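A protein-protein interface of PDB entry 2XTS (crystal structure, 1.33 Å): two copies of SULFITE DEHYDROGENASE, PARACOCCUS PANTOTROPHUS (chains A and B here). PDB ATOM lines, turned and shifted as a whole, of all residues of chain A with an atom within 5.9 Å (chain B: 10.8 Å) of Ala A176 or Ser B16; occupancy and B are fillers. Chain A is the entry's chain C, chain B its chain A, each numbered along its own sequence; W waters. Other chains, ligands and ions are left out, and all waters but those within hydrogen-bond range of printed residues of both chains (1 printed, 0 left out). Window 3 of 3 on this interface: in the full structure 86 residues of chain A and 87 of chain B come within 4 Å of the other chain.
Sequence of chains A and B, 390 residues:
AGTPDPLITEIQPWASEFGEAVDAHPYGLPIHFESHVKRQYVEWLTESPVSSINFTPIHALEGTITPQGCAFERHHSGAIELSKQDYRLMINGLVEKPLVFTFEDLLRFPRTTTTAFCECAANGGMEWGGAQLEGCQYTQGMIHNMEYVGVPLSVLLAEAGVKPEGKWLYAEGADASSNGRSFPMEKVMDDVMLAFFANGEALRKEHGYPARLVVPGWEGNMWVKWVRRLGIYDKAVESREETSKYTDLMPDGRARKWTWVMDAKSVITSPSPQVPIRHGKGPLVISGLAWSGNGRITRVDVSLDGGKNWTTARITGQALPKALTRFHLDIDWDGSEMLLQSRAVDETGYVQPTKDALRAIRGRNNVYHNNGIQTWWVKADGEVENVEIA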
ATOM      1  N   SER A  77     -10.741  15.560  14.172  1.00  0.00           N
ATOM      2  CA  SER A  77     -10.997  15.836  12.745  1.00  0.00           C
ATOM      3  C   SER A  77     -10.119  16.975  12.234  1.00  0.00           C
ATOM      4  O   SER A  77     -10.501  17.714  11.326  1.00  0.00           O
ATOM      5  CB  SER A  77     -12.475  16.125  12.484  1.00  0.00           C
ATOM      6  OG  SER A  77     -12.921  17.272  13.143  1.00  0.00           O
ATOM      7  N   ILE A  80      -8.958  23.094  12.875  1.00  0.00           N
ATOM      8  CA  ILE A  80      -9.779  23.882  11.966  1.00  0.00           C
ATOM      9  C   ILE A  80      -9.460  25.365  12.063  1.00  0.00           C
ATOM     10  O   ILE A  80      -8.963  25.827  13.096  1.00  0.00           O
ATOM     11  CB  ILE A  80     -11.285  23.664  12.216  1.00  0.00           C
ATOM     12  CG1 ILE A  80     -11.689  24.018  13.662  1.00  0.00           C
ATOM     13  CG2 ILE A  80     -11.664  22.216  11.851  1.00  0.00           C
ATOM     14  CD1 ILE A  80     -13.184  24.264  13.851  1.00  0.00           C
ATOM     15  N   ALA A 174     -16.826  23.319  17.246  1.00  0.00           N
ATOM     16  CA  ALA A 174     -17.225  23.706  15.909  1.00  0.00           C
ATOM     17  C   ALA A 174     -16.752  22.734  14.824  1.00  0.00           C
ATOM     18  O   ALA A 174     -17.224  22.822  13.699  1.00  0.00           O
ATOM     19  CB  ALA A 174     -16.742  25.122  15.617  1.00  0.00           C
ATOM     20  N   ASP A 175     -15.815  21.847  15.162  1.00  0.00           N
ATOM     21  CA  ASP A 175     -15.227  20.897  14.239  1.00  0.00           C
ATOM     22  C   ASP A 175     -16.173  19.727  13.939  1.00  0.00           C
ATOM     23  O   ASP A 175     -17.187  19.520  14.599  1.00  0.00           O
ATOM     24  CB  ASP A 175     -13.846  20.436  14.756  1.00  0.00           C
ATOM     25  CG  ASP A 175     -13.876  19.776  16.154  1.00  0.00           C
ATOM     26  OD1 ASP A 175     -14.694  20.185  17.009  1.00  0.00           O
ATOM     27  OD2 ASP A 175     -13.030  18.886  16.423  1.00  0.00           O
ATOM     28  N   ALA A 176     -15.859  18.990  12.888  1.00  0.00           N
ATOM     29  CA  ALA A 176     -16.635  17.837  12.491  1.00  0.00           C
ATOM     30  C   ALA A 176     -16.732  16.816  13.606  1.00  0.00           C
ATOM     31  O   ALA A 176     -17.780  16.210  13.832  1.00  0.00           O
ATOM     32  CB  ALA A 176     -16.031  17.213  11.244  1.00  0.00           C
ATOM     33  N   SER A 177     -15.654  16.649  14.356  1.00  0.00           N
ATOM     34  CA  SER A 177     -15.647  15.637  15.413  1.00  0.00           C
ATOM     35  C   SER A 177     -16.547  15.980  16.590  1.00  0.00           C
ATOM     36  O   SER A 177     -16.920  15.098  17.335  1.00  0.00           O
ATOM     37  CB  SER A 177     -14.226  15.331  15.897  1.00  0.00           C
ATOM     38  OG  SER A 177     -13.800  16.313  16.844  1.00  0.00           O
ATOM     39  N   SER A 178     -16.756  17.284  16.803  1.00  0.00           N
ATOM     40  CA  SER A 178     -17.564  17.857  17.901  1.00  0.00           C
ATOM     41  C   SER A 178     -16.934  17.711  19.280  1.00  0.00           C
ATOM     42  O   SER A 178     -16.964  18.648  20.067  1.00  0.00           O
ATOM     43  CB  SER A 178     -19.023  17.366  17.895  1.00  0.00           C
ATOM     44  OG  SER A 178     -19.315  16.380  18.865  1.00  0.00           O
ATOM     45  N   GLU B  10     -26.568  26.935   8.325  1.00  0.00           N
ATOM     46  CA  GLU B  10     -25.900  26.195   7.266  1.00  0.00           C
ATOM     47  C   GLU B  10     -24.630  25.556   7.828  1.00  0.00           C
ATOM     48  O   GLU B  10     -23.891  26.180   8.586  1.00  0.00           O
ATOM     49  CB  GLU B  10     -25.596  27.116   6.081  1.00  0.00           C
ATOM     50  CG  GLU B  10     -26.891  27.750   5.516  1.00  0.00           C
ATOM     51  CD  GLU B  10     -26.664  28.798   4.437  1.00  0.00           C
ATOM     52  OE1 GLU B  10     -25.501  29.088   4.083  1.00  0.00           O
ATOM     53  OE2 GLU B  10     -27.680  29.318   3.926  1.00  0.00           O
ATOM     54  N   ILE B  11     -24.399  24.304   7.462  1.00  0.00           N
ATOM     55  CA  ILE B  11     -23.203  23.557   7.894  1.00  0.00           C
ATOM     56  C   ILE B  11     -21.979  24.193   7.233  1.00  0.00           C
ATOM     57  O   ILE B  11     -21.953  24.375   6.011  1.00  0.00           O
ATOM     58  CB  ILE B  11     -23.311  22.071   7.533  1.00  0.00           C
ATOM     59  CG1 ILE B  11     -24.498  21.421   8.257  1.00  0.00           C
ATOM     60  CG2 ILE B  11     -21.988  21.329   7.858  1.00  0.00           C
ATOM     61  CD1 ILE B  11     -24.963  20.111   7.609  1.00  0.00           C
ATOM     62  N   GLN B  12     -20.986  24.587   8.030  1.00  0.00           N
ATOM     63  CA  GLN B  12     -19.786  25.234   7.497  1.00  0.00           C
ATOM     64  C   GLN B  12     -18.736  24.168   7.218  1.00  0.00           C
ATOM     65  O   GLN B  12     -18.769  23.098   7.798  1.00  0.00           O
ATOM     66  CB  GLN B  12     -19.283  26.290   8.484  1.00  0.00           C
ATOM     67  CG  GLN B  12     -20.348  27.346   8.804  1.00  0.00           C
ATOM     68  CD  GLN B  12     -20.777  28.096   7.553  1.00  0.00           C
ATOM     69  OE1 GLN B  12     -19.948  28.441   6.716  1.00  0.00           O
ATOM     70  NE2 GLN B  12     -22.070  28.325   7.414  1.00  0.00           N
ATOM     71  N   PRO B  13     -17.791  24.462   6.323  1.00  0.00           N
ATOM     72  CA  PRO B  13     -16.834  23.421   5.936  1.00  0.00           C
ATOM     73  C   PRO B  13     -16.050  22.843   7.108  1.00  0.00           C
ATOM     74  O   PRO B  13     -15.751  21.657   7.114  1.00  0.00           O
ATOM     75  CB  PRO B  13     -15.915  24.131   4.937  1.00  0.00           C
ATOM     76  CG  PRO B  13     -16.722  25.233   4.417  1.00  0.00           C
ATOM     77  CD  PRO B  13     -17.667  25.662   5.481  1.00  0.00           C
ATOM     78  N   TRP B  14     -15.710  23.674   8.088  1.00  0.00           N
ATOM     79  CA  TRP B  14     -14.932  23.232   9.238  1.00  0.00           C
ATOM     80  C   TRP B  14     -15.704  22.289  10.148  1.00  0.00           C
ATOM     81  O   TRP B  14     -15.106  21.671  11.034  1.00  0.00           O
ATOM     82  CB  TRP B  14     -14.419  24.447  10.016  1.00  0.00           C
ATOM     83  CG  TRP B  14     -15.456  25.405  10.496  1.00  0.00           C
ATOM     84  CD1 TRP B  14     -16.198  25.320  11.631  1.00  0.00           C
ATOM     85  CD2 TRP B  14     -15.859  26.609   9.851  1.00  0.00           C
ATOM     86  NE1 TRP B  14     -17.033  26.411  11.740  1.00  0.00           N
ATOM     87  CE2 TRP B  14     -16.837  27.220  10.656  1.00  0.00           C
ATOM     88  CE3 TRP B  14     -15.469  27.249   8.675  1.00  0.00           C
ATOM     89  CZ2 TRP B  14     -17.437  28.432  10.305  1.00  0.00           C
ATOM     90  CZ3 TRP B  14     -16.073  28.446   8.330  1.00  0.00           C
ATOM     91  CH2 TRP B  14     -17.036  29.022   9.137  1.00  0.00           C
ATOM     92  N   ALA B  15     -17.021  22.173   9.951  1.00  0.00           N
ATOM     93  CA  ALA B  15     -17.862  21.250  10.744  1.00  0.00           C
ATOM     94  C   ALA B  15     -18.169  19.968   9.987  1.00  0.00           C
ATOM     95  O   ALA B  15     -19.008  19.184  10.423  1.00  0.00           O
ATOM     96  CB  ALA B  15     -19.151  21.951  11.167  1.00  0.00           C
ATOM     97  N   SER B  16     -17.476  19.761   8.861  1.00  0.00           N
ATOM     98  CA  SER B  16     -17.726  18.596   8.010  1.00  0.00           C
ATOM     99  C   SER B  16     -16.442  17.949   7.515  1.00  0.00           C
ATOM    100  O   SER B  16     -16.246  16.745   7.652  1.00  0.00           O
ATOM    101  CB  SER B  16     -18.600  18.992   6.818  1.00  0.00           C
ATOM    102  OG  SER B  16     -18.860  17.891   5.975  1.00  0.00           O
ATOM    103  N   GLU B  17     -15.582  18.774   6.923  1.00  0.00           N
ATOM    104  CA  GLU B  17     -14.307  18.361   6.366  1.00  0.00           C
ATOM    105  C   GLU B  17     -13.229  18.359   7.438  1.00  0.00           C
ATOM    106  O   GLU B  17     -13.429  18.859   8.518  1.00  0.00           O
ATOM    107  CB  GLU B  17     -13.894  19.342   5.249  1.00  0.00           C
ATOM    108  CG  GLU B  17     -14.848  19.394   4.060  1.00  0.00           C
ATOM    109  CD  GLU B  17     -14.657  20.634   3.194  1.00  0.00           C
ATOM    110  OE1 GLU B  17     -13.583  21.262   3.251  1.00  0.00           O
ATOM    111  OE2 GLU B  17     -15.607  20.992   2.468  1.00  0.00           O
ATOM    112  N   PHE B  18     -12.050  17.890   7.091  1.00  0.00           N
ATOM    113  CA  PHE B  18     -10.922  17.851   8.005  1.00  0.00           C
ATOM    114  C   PHE B  18     -10.247  19.207   8.106  1.00  0.00           C
ATOM    115  O   PHE B  18     -10.150  19.946   7.120  1.00  0.00           O
ATOM    116  CB  PHE B  18      -9.823  16.904   7.524  1.00  0.00           C
ATOM    117  CG  PHE B  18     -10.208  15.464   7.447  1.00  0.00           C
ATOM    118  CD1 PHE B  18     -11.025  14.865   8.376  1.00  0.00           C
ATOM    119  CD2 PHE B  18      -9.674  14.690   6.449  1.00  0.00           C
ATOM    120  CE1 PHE B  18     -11.321  13.512   8.284  1.00  0.00           C
ATOM    121  CE2 PHE B  18      -9.955  13.345   6.355  1.00  0.00           C
ATOM    122  CZ  PHE B  18     -10.778  12.760   7.268  1.00  0.00           C
ATOM    123  N   GLY B  19      -9.723  19.485   9.301  1.00  0.00           N
ATOM    124  CA  GLY B  19      -8.724  20.512   9.512  1.00  0.00           C
ATOM    125  C   GLY B  19      -7.323  19.966   9.214  1.00  0.00           C
ATOM    126  O   GLY B  19      -7.178  18.876   8.667  1.00  0.00           O
ATOM    127  N   GLU B  20      -6.290  20.690   9.623  1.00  0.00           N
ATOM    128  CA  GLU B  20      -4.908  20.234   9.424  1.00  0.00           C
ATOM    129  C   GLU B  20      -4.521  19.073  10.353  1.00  0.00           C
ATOM    130  O   GLU B  20      -4.983  18.947  11.483  1.00  0.00           O
ATOM    131  CB  GLU B  20      -3.914  21.371   9.631  1.00  0.00           C
ATOM    132  CG  GLU B  20      -4.008  22.505   8.600  1.00  0.00           C
ATOM    133  CD  GLU B  20      -2.877  23.501   8.793  1.00  0.00           C
ATOM    134  OE1 GLU B  20      -3.029  24.394   9.641  1.00  0.00           O
ATOM    135  OE2 GLU B  20      -1.824  23.368   8.133  1.00  0.00           O
HETATM  136  O   HOH W   1     -13.424  19.407  11.212  1.00  0.00           O
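The backbone carbonyl oxygen of Trp B14 sits at hydrogen-bond distance from the backbone NH of Ala A176.
The backbone NH of Gly B19 is in hydrogen-bond range of the backbone carbonyl oxygen of Ser A77, at 2.8 Å.
OG of Ser A77 is in hydrogen-bond range of N of Ala A176.
OG of Ser A77 lies within hydrogen-bond range of N of Ser A177.
The side-chain carboxylate (OD2) of Asp A175 lies within hydrogen-bond range of the side-chain hydroxyl (OG) of Ser A177 (2.7 Å).
O of Ser A77 touches CA of Phe B18, at 3.4 Å.
Ile A80 touches Trp B14.
Ala A174 touches Trp B14.
Ala A174 touches Ala B15 (O to CB, 3.3 Å).
O of Trp B14 touches CA of Asp A175, 3.3 Å away.
Ala B15 touches Asp A175.
Ala A176 touches Ala B15 (CA to O, 3.4 Å).
Ser B16 touches Ala A176.
Ser B16 touches one residue of chain A.
Printed residues of chain B within 4 Å of Ser A77: Phe B18 and Gly B19.
Of the printed residues of chain B, Asp A175 touches Trp B14 (3.3 Å) and Ala B15 (3.9 Å).
No residue of chain B comes within 4 Å of Ser A177.
Of the printed residues of chain A, Trp B14 touches Ile A80 (3.6 Å), Ala A174 (3.4 Å), Asp A175 (3.3 Å) and Ala A176 (3.3 Å).
Of the printed residues of chain A, Gly B19 touches Ser A77 (2.8 Å).
Printed residues of chain A within 4 Å of Phe B18: Ser A77 (3.4 Å).
Printed residues of chain A within 4 Å of Ala B15: Ala A174 (3.3 Å), Asp A175 (3.9 Å) and Ala A176 (3.4 Å).
Of the printed residues of chain B, Ile A80 touches Trp B14 (3.6 Å).
The nearest printed residue of chain A that does not touch Ala B15 is Ile A80 (5.7 Å).
Of the 11 printed residues of chain B, 5 touch a printed residue of chain A.
Printed residues of chain B that touch a printed residue of chain A: Trp B14, Ala B15, Ser B16, Phe B18 and Gly B19.
Of the 7 printed residues of chain A, 5 touch a printed residue of chain B.
Hydrophobic or aromatic side chains of chain A that line the printed part of chain B: Ile A80 and Ala A176.
Among the printed residues, 10 pairs touch across the chains.
Among the printed residues, no Asp or Glu carboxylate lies within 4 Å of a Lys or Arg side-chain nitrogen of the other chain.
No position is printed for both chains.
Of the 10 pairs that touch across the chains among the printed residues, none has its exchanged pair printed and touching as well.
Water W1 lies within hydrogen-bond range of O of Glu B17 (2.7 Å), O of Trp B14 (2.8 Å), OG of Ser A77 (2.9 Å) and N of Ala A176 (3.0 Å).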
